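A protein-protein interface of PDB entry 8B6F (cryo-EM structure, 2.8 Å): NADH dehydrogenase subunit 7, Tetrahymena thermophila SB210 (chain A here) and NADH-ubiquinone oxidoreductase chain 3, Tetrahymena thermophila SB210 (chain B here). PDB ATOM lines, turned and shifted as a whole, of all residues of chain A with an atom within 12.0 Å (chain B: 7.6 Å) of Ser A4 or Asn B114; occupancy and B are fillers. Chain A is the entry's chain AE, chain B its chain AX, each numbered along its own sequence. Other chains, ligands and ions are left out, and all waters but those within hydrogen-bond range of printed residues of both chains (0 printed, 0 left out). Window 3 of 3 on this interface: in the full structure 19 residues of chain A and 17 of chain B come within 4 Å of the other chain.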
ATOM      1  N   MET A   1      31.086 -31.817  32.695  1.00  0.00           N
ATOM      2  CA  MET A   1      30.521 -31.413  31.376  1.00  0.00           C
ATOM      3  C   MET A   1      29.951 -32.619  30.641  1.00  0.00           C
ATOM      4  O   MET A   1      30.603 -33.656  30.535  1.00  0.00           O
ATOM      5  CB  MET A   1      31.591 -30.737  30.518  1.00  0.00           C
ATOM      6  CG  MET A   1      32.188 -29.487  31.147  1.00  0.00           C
ATOM      7  SD  MET A   1      33.512 -28.761  30.161  1.00  0.00           S
ATOM      8  CE  MET A   1      32.643 -28.356  28.648  1.00  0.00           C
ATOM      9  N   ASN A   2      28.732 -32.475  30.135  1.00  0.00           N
ATOM     10  CA  ASN A   2      28.063 -33.545  29.415  1.00  0.00           C
ATOM     11  C   ASN A   2      28.405 -33.485  27.928  1.00  0.00           C
ATOM     12  O   ASN A   2      29.025 -32.538  27.440  1.00  0.00           O
ATOM     13  CB  ASN A   2      26.551 -33.459  29.616  1.00  0.00           C
ATOM     14  CG  ASN A   2      26.159 -33.440  31.080  1.00  0.00           C
ATOM     15  OD1 ASN A   2      26.960 -33.091  31.943  1.00  0.00           O
ATOM     16  ND2 ASN A   2      24.918 -33.816  31.365  1.00  0.00           N
ATOM     17  N   ARG A   3      27.989 -34.519  27.204  1.00  0.00           N
ATOM     18  CA  ARG A   3      28.261 -34.593  25.776  1.00  0.00           C
ATOM     19  C   ARG A   3      27.465 -33.537  25.018  1.00  0.00           C
ATOM     20  O   ARG A   3      26.376 -33.129  25.429  1.00  0.00           O
ATOM     21  CB  ARG A   3      27.915 -35.975  25.227  1.00  0.00           C
ATOM     22  CG  ARG A   3      28.527 -37.134  25.988  1.00  0.00           C
ATOM     23  CD  ARG A   3      28.379 -38.422  25.194  1.00  0.00           C
ATOM     24  NE  ARG A   3      28.615 -39.610  26.005  1.00  0.00           N
ATOM     25  CZ  ARG A   3      27.674 -40.273  26.664  1.00  0.00           C
ATOM     26  NH1 ARG A   3      26.410 -39.883  26.646  1.00  0.00           N
ATOM     27  NH2 ARG A   3      28.009 -41.359  27.354  1.00  0.00           N
ATOM     28  N   SER A   4      28.033 -33.087  23.895  1.00  0.00           N
ATOM     29  CA  SER A   4      27.340 -32.159  23.009  1.00  0.00           C
ATOM     30  C   SER A   4      27.573 -32.498  21.541  1.00  0.00           C
ATOM     31  O   SER A   4      27.416 -31.624  20.681  1.00  0.00           O
ATOM     32  CB  SER A   4      27.784 -30.719  23.274  1.00  0.00           C
ATOM     33  OG  SER A   4      27.492 -30.329  24.604  1.00  0.00           O
ATOM     34  N   ILE A   5      27.930 -33.745  21.231  1.00  0.00           N
ATOM     35  CA  ILE A   5      28.268 -34.101  19.855  1.00  0.00           C
ATOM     36  C   ILE A   5      27.073 -33.876  18.937  1.00  0.00           C
ATOM     37  O   ILE A   5      27.213 -33.335  17.834  1.00  0.00           O
ATOM     38  CB  ILE A   5      28.780 -35.554  19.791  1.00  0.00           C
ATOM     39  CG1 ILE A   5      29.200 -35.925  18.364  1.00  0.00           C
ATOM     40  CG2 ILE A   5      27.728 -36.531  20.297  1.00  0.00           C
ATOM     41  CD1 ILE A   5      30.368 -35.123  17.831  1.00  0.00           C
ATOM     42  N   PHE A   6      25.880 -34.279  19.376  1.00  0.00           N
ATOM     43  CA  PHE A   6      24.697 -34.134  18.535  1.00  0.00           C
ATOM     44  C   PHE A   6      24.343 -32.671  18.309  1.00  0.00           C
ATOM     45  O   PHE A   6      23.841 -32.315  17.237  1.00  0.00           O
ATOM     46  CB  PHE A   6      23.519 -34.879  19.154  1.00  0.00           C
ATOM     47  CG  PHE A   6      23.758 -36.349  19.312  1.00  0.00           C
ATOM     48  CD1 PHE A   6      23.795 -37.181  18.207  1.00  0.00           C
ATOM     49  CD2 PHE A   6      23.937 -36.902  20.567  1.00  0.00           C
ATOM     50  CE1 PHE A   6      24.015 -38.535  18.350  1.00  0.00           C
ATOM     51  CE2 PHE A   6      24.154 -38.254  20.716  1.00  0.00           C
ATOM     52  CZ  PHE A   6      24.192 -39.073  19.605  1.00  0.00           C
ATOM     53  N   GLN A   7      24.585 -31.815  19.299  1.00  0.00           N
ATOM     54  CA  GLN A   7      24.383 -30.386  19.115  1.00  0.00           C
ATOM     55  C   GLN A   7      25.499 -29.742  18.307  1.00  0.00           C
ATOM     56  O   GLN A   7      25.324 -28.620  17.821  1.00  0.00           O
ATOM     57  CB  GLN A   7      24.278 -29.690  20.474  1.00  0.00           C
ATOM     58  CG  GLN A   7      23.213 -30.268  21.385  1.00  0.00           C
ATOM     59  CD  GLN A   7      23.137 -29.547  22.713  1.00  0.00           C
ATOM     60  OE1 GLN A   7      23.536 -28.389  22.827  1.00  0.00           O
ATOM     61  NE2 GLN A   7      22.629 -30.233  23.731  1.00  0.00           N
ATOM     62  N   LEU A   8      26.633 -30.423  18.148  1.00  0.00           N
ATOM     63  CA  LEU A   8      27.789 -29.846  17.476  1.00  0.00           C
ATOM     64  C   LEU A   8      27.928 -30.255  16.016  1.00  0.00           C
ATOM     65  O   LEU A   8      28.599 -29.546  15.262  1.00  0.00           O
ATOM     66  CB  LEU A   8      29.073 -30.232  18.220  1.00  0.00           C
ATOM     67  CG  LEU A   8      29.317 -29.521  19.553  1.00  0.00           C
ATOM     68  CD1 LEU A   8      30.502 -30.143  20.266  1.00  0.00           C
ATOM     69  CD2 LEU A   8      29.537 -28.032  19.350  1.00  0.00           C
ATOM     70  N   TRP A   9      27.332 -31.370  15.595  1.00  0.00           N
ATOM     71  CA  TRP A   9      27.427 -31.801  14.207  1.00  0.00           C
ATOM     72  C   TRP A   9      26.059 -32.244  13.709  1.00  0.00           C
ATOM     73  O   TRP A   9      25.229 -32.737  14.477  1.00  0.00           O
ATOM     74  CB  TRP A   9      28.463 -32.927  14.050  1.00  0.00           C
ATOM     75  CG  TRP A   9      27.915 -34.323  14.098  1.00  0.00           C
ATOM     76  CD1 TRP A   9      27.107 -34.859  15.057  1.00  0.00           C
ATOM     77  CD2 TRP A   9      28.161 -35.369  13.151  1.00  0.00           C
ATOM     78  NE1 TRP A   9      26.827 -36.170  14.761  1.00  0.00           N
ATOM     79  CE2 TRP A   9      27.461 -36.506  13.594  1.00  0.00           C
ATOM     80  CE3 TRP A   9      28.899 -35.450  11.966  1.00  0.00           C
ATOM     81  CZ2 TRP A   9      27.477 -37.711  12.896  1.00  0.00           C
ATOM     82  CZ3 TRP A   9      28.915 -36.648  11.273  1.00  0.00           C
ATOM     83  CH2 TRP A   9      28.206 -37.762  11.740  1.00  0.00           C
ATOM     84  N   LYS A  10      25.831 -32.053  12.410  1.00  0.00           N
ATOM     85  CA  LYS A  10      24.573 -32.430  11.767  1.00  0.00           C
ATOM     86  C   LYS A  10      24.890 -33.129  10.450  1.00  0.00           C
ATOM     87  O   LYS A  10      25.159 -32.462   9.439  1.00  0.00           O
ATOM     88  CB  LYS A  10      23.681 -31.215  11.531  1.00  0.00           C
ATOM     89  CG  LYS A  10      22.429 -31.529  10.728  1.00  0.00           C
ATOM     90  CD  LYS A  10      21.510 -30.327  10.620  1.00  0.00           C
ATOM     91  CE  LYS A  10      20.306 -30.646   9.747  1.00  0.00           C
ATOM     92  NZ  LYS A  10      19.401 -29.477   9.580  1.00  0.00           N
ATOM     93  N   PRO A  11      24.866 -34.457  10.415  1.00  0.00           N
ATOM     94  CA  PRO A  11      25.140 -35.170   9.165  1.00  0.00           C
ATOM     95  C   PRO A  11      23.940 -35.130   8.227  1.00  0.00           C
ATOM     96  O   PRO A  11      22.834 -34.736   8.594  1.00  0.00           O
ATOM     97  CB  PRO A  11      25.431 -36.598   9.633  1.00  0.00           C
ATOM     98  CG  PRO A  11      24.627 -36.742  10.861  1.00  0.00           C
ATOM     99  CD  PRO A  11      24.626 -35.392  11.529  1.00  0.00           C
ATOM    100  N   ILE A  51      28.397 -19.221  10.532  1.00  0.00           N
ATOM    101  CA  ILE A  51      29.456 -20.214  10.651  1.00  0.00           C
ATOM    102  C   ILE A  51      29.791 -20.695   9.247  1.00  0.00           C
ATOM    103  O   ILE A  51      28.913 -21.183   8.526  1.00  0.00           O
ATOM    104  CB  ILE A  51      29.036 -21.385  11.553  1.00  0.00           C
ATOM    105  CG1 ILE A  51      28.778 -20.881  12.973  1.00  0.00           C
ATOM    106  CG2 ILE A  51      30.105 -22.470  11.553  1.00  0.00           C
ATOM    107  CD1 ILE A  51      28.232 -21.927  13.915  1.00  0.00           C
ATOM    108  N   MET B  63      17.544 -20.464  22.109  1.00  0.00           N
ATOM    109  CA  MET B  63      17.369 -20.768  23.524  1.00  0.00           C
ATOM    110  C   MET B  63      17.742 -19.581  24.396  1.00  0.00           C
ATOM    111  O   MET B  63      17.149 -19.382  25.463  1.00  0.00           O
ATOM    112  CB  MET B  63      18.209 -21.985  23.909  1.00  0.00           C
ATOM    113  CG  MET B  63      17.775 -23.276  23.239  1.00  0.00           C
ATOM    114  SD  MET B  63      16.042 -23.687  23.527  1.00  0.00           S
ATOM    115  CE  MET B  63      15.972 -23.697  25.315  1.00  0.00           C
ATOM    116  N   PHE B  67      15.230 -18.046  27.129  1.00  0.00           N
ATOM    117  CA  PHE B  67      15.546 -17.875  28.540  1.00  0.00           C
ATOM    118  C   PHE B  67      15.535 -16.411  28.946  1.00  0.00           C
ATOM    119  O   PHE B  67      15.229 -16.093  30.100  1.00  0.00           O
ATOM    120  CB  PHE B  67      16.903 -18.507  28.850  1.00  0.00           C
ATOM    121  CG  PHE B  67      16.926 -19.999  28.682  1.00  0.00           C
ATOM    122  CD1 PHE B  67      15.861 -20.779  29.104  1.00  0.00           C
ATOM    123  CD2 PHE B  67      18.012 -20.622  28.095  1.00  0.00           C
ATOM    124  CE1 PHE B  67      15.881 -22.147  28.947  1.00  0.00           C
ATOM    125  CE2 PHE B  67      18.038 -21.988  27.936  1.00  0.00           C
ATOM    126  CZ  PHE B  67      16.971 -22.754  28.363  1.00  0.00           C
ATOM    127  N   LEU B 108      21.520 -22.943  36.588  1.00  0.00           N
ATOM    128  CA  LEU B 108      22.394 -24.103  36.723  1.00  0.00           C
ATOM    129  C   LEU B 108      21.908 -25.263  35.865  1.00  0.00           C
ATOM    130  O   LEU B 108      22.712 -25.951  35.225  1.00  0.00           O
ATOM    131  CB  LEU B 108      22.485 -24.520  38.192  1.00  0.00           C
ATOM    132  CG  LEU B 108      23.330 -25.761  38.494  1.00  0.00           C
ATOM    133  CD1 LEU B 108      24.765 -25.569  38.035  1.00  0.00           C
ATOM    134  CD2 LEU B 108      23.281 -26.083  39.976  1.00  0.00           C
ATOM    135  N   TYR B 109      20.595 -25.492  35.831  1.00  0.00           N
ATOM    136  CA  TYR B 109      20.053 -26.552  34.988  1.00  0.00           C
ATOM    137  C   TYR B 109      20.317 -26.269  33.516  1.00  0.00           C
ATOM    138  O   TYR B 109      20.664 -27.177  32.754  1.00  0.00           O
ATOM    139  CB  TYR B 109      18.556 -26.714  35.242  1.00  0.00           C
ATOM    140  CG  TYR B 109      17.924 -27.823  34.434  1.00  0.00           C
ATOM    141  CD1 TYR B 109      17.975 -29.141  34.869  1.00  0.00           C
ATOM    142  CD2 TYR B 109      17.276 -27.552  33.238  1.00  0.00           C
ATOM    143  CE1 TYR B 109      17.400 -30.156  34.135  1.00  0.00           C
ATOM    144  CE2 TYR B 109      16.698 -28.561  32.496  1.00  0.00           C
ATOM    145  CZ  TYR B 109      16.762 -29.861  32.950  1.00  0.00           C
ATOM    146  OH  TYR B 109      16.188 -30.870  32.215  1.00  0.00           O
ATOM    147  N   ASP B 110      20.154 -25.014  33.094  1.00  0.00           N
ATOM    148  CA  ASP B 110      20.464 -24.659  31.714  1.00  0.00           C
ATOM    149  C   ASP B 110      21.924 -24.953  31.394  1.00  0.00           C
ATOM    150  O   ASP B 110      22.236 -25.514  30.337  1.00  0.00           O
ATOM    151  CB  ASP B 110      20.148 -23.184  31.470  1.00  0.00           C
ATOM    152  CG  ASP B 110      18.686 -22.856  31.706  1.00  0.00           C
ATOM    153  OD1 ASP B 110      17.837 -23.748  31.507  1.00  0.00           O
ATOM    154  OD2 ASP B 110      18.385 -21.706  32.087  1.00  0.00           O
ATOM    155  N   TRP B 111      22.835 -24.582  32.295  1.00  0.00           N
ATOM    156  CA  TRP B 111      24.249 -24.871  32.079  1.00  0.00           C
ATOM    157  C   TRP B 111      24.499 -26.371  31.994  1.00  0.00           C
ATOM    158  O   TRP B 111      25.250 -26.834  31.128  1.00  0.00           O
ATOM    159  CB  TRP B 111      25.101 -24.253  33.188  1.00  0.00           C
ATOM    160  CG  TRP B 111      26.562 -24.481  32.971  1.00  0.00           C
ATOM    161  CD1 TRP B 111      27.435 -23.638  32.355  1.00  0.00           C
ATOM    162  CD2 TRP B 111      27.323 -25.631  33.366  1.00  0.00           C
ATOM    163  NE1 TRP B 111      28.691 -24.190  32.336  1.00  0.00           N
ATOM    164  CE2 TRP B 111      28.649 -25.415  32.947  1.00  0.00           C
ATOM    165  CE3 TRP B 111      27.010 -26.823  34.026  1.00  0.00           C
ATOM    166  CZ2 TRP B 111      29.665 -26.338  33.180  1.00  0.00           C
ATOM    167  CZ3 TRP B 111      28.021 -27.744  34.250  1.00  0.00           C
ATOM    168  CH2 TRP B 111      29.333 -27.496  33.828  1.00  0.00           C
ATOM    169  N   LEU B 112      23.875 -27.148  32.879  1.00  0.00           N
ATOM    170  CA  LEU B 112      24.081 -28.593  32.867  1.00  0.00           C
ATOM    171  C   LEU B 112      23.654 -29.200  31.539  1.00  0.00           C
ATOM    172  O   LEU B 112      24.347 -30.066  30.994  1.00  0.00           O
ATOM    173  CB  LEU B 112      23.305 -29.241  34.015  1.00  0.00           C
ATOM    174  CG  LEU B 112      23.816 -28.999  35.436  1.00  0.00           C
ATOM    175  CD1 LEU B 112      22.828 -29.539  36.452  1.00  0.00           C
ATOM    176  CD2 LEU B 112      25.175 -29.636  35.636  1.00  0.00           C
ATOM    177  N   ASN B 113      22.519 -28.765  31.002  1.00  0.00           N
ATOM    178  CA  ASN B 113      22.027 -29.298  29.739  1.00  0.00           C
ATOM    179  C   ASN B 113      22.710 -28.685  28.523  1.00  0.00           C
ATOM    180  O   ASN B 113      22.506 -29.178  27.409  1.00  0.00           O
ATOM    181  CB  ASN B 113      20.518 -29.090  29.644  1.00  0.00           C
ATOM    182  CG  ASN B 113      19.747 -30.155  30.387  1.00  0.00           C
ATOM    183  OD1 ASN B 113      19.256 -31.111  29.791  1.00  0.00           O
ATOM    184  ND2 ASN B 113      19.647 -30.000  31.701  1.00  0.00           N
ATOM    185  N   ASN B 114      23.510 -27.636  28.702  1.00  0.00           N
ATOM    186  CA  ASN B 114      24.322 -27.074  27.623  1.00  0.00           C
ATOM    187  C   ASN B 114      23.444 -26.517  26.505  1.00  0.00           C
ATOM    188  O   ASN B 114      23.661 -26.778  25.321  1.00  0.00           O
ATOM    189  CB  ASN B 114      25.303 -28.112  27.075  1.00  0.00           C
ATOM    190  CG  ASN B 114      26.222 -28.665  28.145  1.00  0.00           C
ATOM    191  OD1 ASN B 114      26.346 -29.878  28.306  1.00  0.00           O
ATOM    192  ND2 ASN B 114      26.868 -27.773  28.889  1.00  0.00           N
ATOM    193  N   VAL B 115      22.435 -25.737  26.898  1.00  0.00           N
ATOM    194  CA  VAL B 115      21.553 -25.076  25.947  1.00  0.00           C
ATOM    195  C   VAL B 115      21.907 -23.610  25.760  1.00  0.00           C
ATOM    196  O   VAL B 115      21.194 -22.893  25.048  1.00  0.00           O
ATOM    197  CB  VAL B 115      20.074 -25.211  26.371  1.00  0.00           C
ATOM    198  CG1 VAL B 115      19.608 -26.646  26.207  1.00  0.00           C
ATOM    199  CG2 VAL B 115      19.880 -24.753  27.810  1.00  0.00           C
ATOM    200  N   LEU B 116      22.996 -23.144  26.374  1.00  0.00           N
ATOM    201  CA  LEU B 116      23.426 -21.754  26.297  1.00  0.00           C
ATOM    202  C   LEU B 116      24.545 -21.554  25.281  1.00  0.00           C
ATOM    203  O   LEU B 116      25.356 -20.635  25.425  1.00  0.00           O
ATOM    204  CB  LEU B 116      23.872 -21.267  27.675  1.00  0.00           C
ATOM    205  CG  LEU B 116      22.863 -21.427  28.815  1.00  0.00           C
ATOM    206  CD1 LEU B 116      23.486 -21.024  30.139  1.00  0.00           C
ATOM    207  CD2 LEU B 116      21.609 -20.611  28.546  1.00  0.00           C
ATOM    208  N   SER B 117      24.610 -22.401  24.256  1.00  0.00           N
ATOM    209  CA  SER B 117      25.664 -22.328  23.258  1.00  0.00           C
ATOM    210  C   SER B 117      25.081 -22.625  21.884  1.00  0.00           C
ATOM    211  O   SER B 117      24.006 -23.213  21.756  1.00  0.00           O
ATOM    212  CB  SER B 117      26.805 -23.306  23.570  1.00  0.00           C
ATOM    213  OG  SER B 117      26.330 -24.640  23.631  1.00  0.00           O
ATOM    214  N   TRP B 118      25.813 -22.207  20.854  1.00  0.00           N
ATOM    215  CA  TRP B 118      25.379 -22.439  19.483  1.00  0.00           C
ATOM    216  C   TRP B 118      25.349 -23.931  19.177  1.00  0.00           C
ATOM    217  O   TRP B 118      26.193 -24.699  19.648  1.00  0.00           O
ATOM    218  CB  TRP B 118      26.315 -21.719  18.511  1.00  0.00           C
ATOM    219  CG  TRP B 118      25.912 -20.306  18.228  1.00  0.00           C
ATOM    220  CD1 TRP B 118      25.558 -19.786  17.019  1.00  0.00           C
ATOM    221  CD2 TRP B 118      25.816 -19.231  19.171  1.00  0.00           C
ATOM    222  NE1 TRP B 118      25.249 -18.453  17.150  1.00  0.00           N
ATOM    223  CE2 TRP B 118      25.399 -18.090  18.462  1.00  0.00           C
ATOM    224  CE3 TRP B 118      26.042 -19.125  20.547  1.00  0.00           C
ATOM    225  CZ2 TRP B 118      25.204 -16.856  19.079  1.00  0.00           C
ATOM    226  CZ3 TRP B 118      25.847 -17.901  21.160  1.00  0.00           C
ATOM    227  CH2 TRP B 118      25.432 -16.781  20.426  1.00  0.00           C
ATOM    228  N   SER B 119      24.364 -24.340  18.383  1.00  0.00           N
ATOM    229  CA  SER B 119      24.164 -25.731  18.013  1.00  0.00           C
ATOM    230  C   SER B 119      24.241 -25.878  16.499  1.00  0.00           C
ATOM    231  O   SER B 119      24.263 -24.896  15.755  1.00  0.00           O
ATOM    232  CB  SER B 119      22.818 -26.250  18.533  1.00  0.00           C
ATOM    233  OG  SER B 119      21.743 -25.474  18.034  1.00  0.00           O
ATOM    234  N   ALA B 120      24.281 -27.134  16.048  1.00  0.00           N
ATOM    235  CA  ALA B 120      24.424 -27.402  14.620  1.00  0.00           C
ATOM    236  C   ALA B 120      23.266 -26.813  13.826  1.00  0.00           C
ATOM    237  O   ALA B 120      23.471 -26.231  12.754  1.00  0.00           O
ATOM    238  CB  ALA B 120      24.525 -28.906  14.378  1.00  0.00           C
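OE1 of Gln A7 lies close to O of Asn B114. The backbone carbonyl oxygen (O) of Gln A7 lies within hydrogen-bond range of the backbone NH (N) of Ala B120, at 2.5 Å.
The backbone carbonyl oxygen (O) of Tyr B109 sits close to the side-chain amide nitrogen (ND2) of Asn B113 (3.2 Å). O of Trp B111 is in hydrogen-bond range of ND2 of Asn B114, at 2.9 Å. The side-chain amide oxygen (OD1) of Asn B114 lies close to the backbone carbonyl oxygen (O) of Leu B112 (3.4 Å).
Among the printed residues, pairs that only touch across the chains: Asn A2 with Leu B112 (3.8 Å), Asn A2 with Asn B114 (3.8 Å), Ser A4 with Asn B114 (3.9 Å), Gln A7 with Asn B113 (3.8 Å), Gln A7 with Ser B119 (3.1 Å), Trp A9 with Ala B120 (3.7 Å) and Lys A10 with Ala B120 (3.8 Å).
Ser A4 touches one residue of chain B. No residue of chain A comes within 4 Å of Trp B111. No residue of chain A comes within 4 Å of Val B115. Of the printed residues of chain B, Trp A9 touches Ala B120 (3.7 Å). Of the printed residues of chain B, Lys A10 touches Ala B120. Of the printed residues of chain A, Ser B119 touches Gln A7 (3.1 Å). Printed residues of chain A within 4 Å of Leu B112: Asn A2. Phe A6 touches none of the printed residues of chain B. The nearest printed residue of chain B that does not touch Trp A9 is Ser B119 (6.4 Å).
Printed residues of chain A that touch a printed residue of chain B: Asn A2, Ser A4, Gln A7, Trp A9 and Lys A10. Hydrophobic or aromatic side chains of chain B that line the printed part of chain A: Ala B120. Along chain B the printed residues that touch a printed residue of chain A span positions 112 to 120. Among the printed residues, no Asp or Glu carboxylate lies within 4 Å of a Lys or Arg side-chain nitrogen of the other chain.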
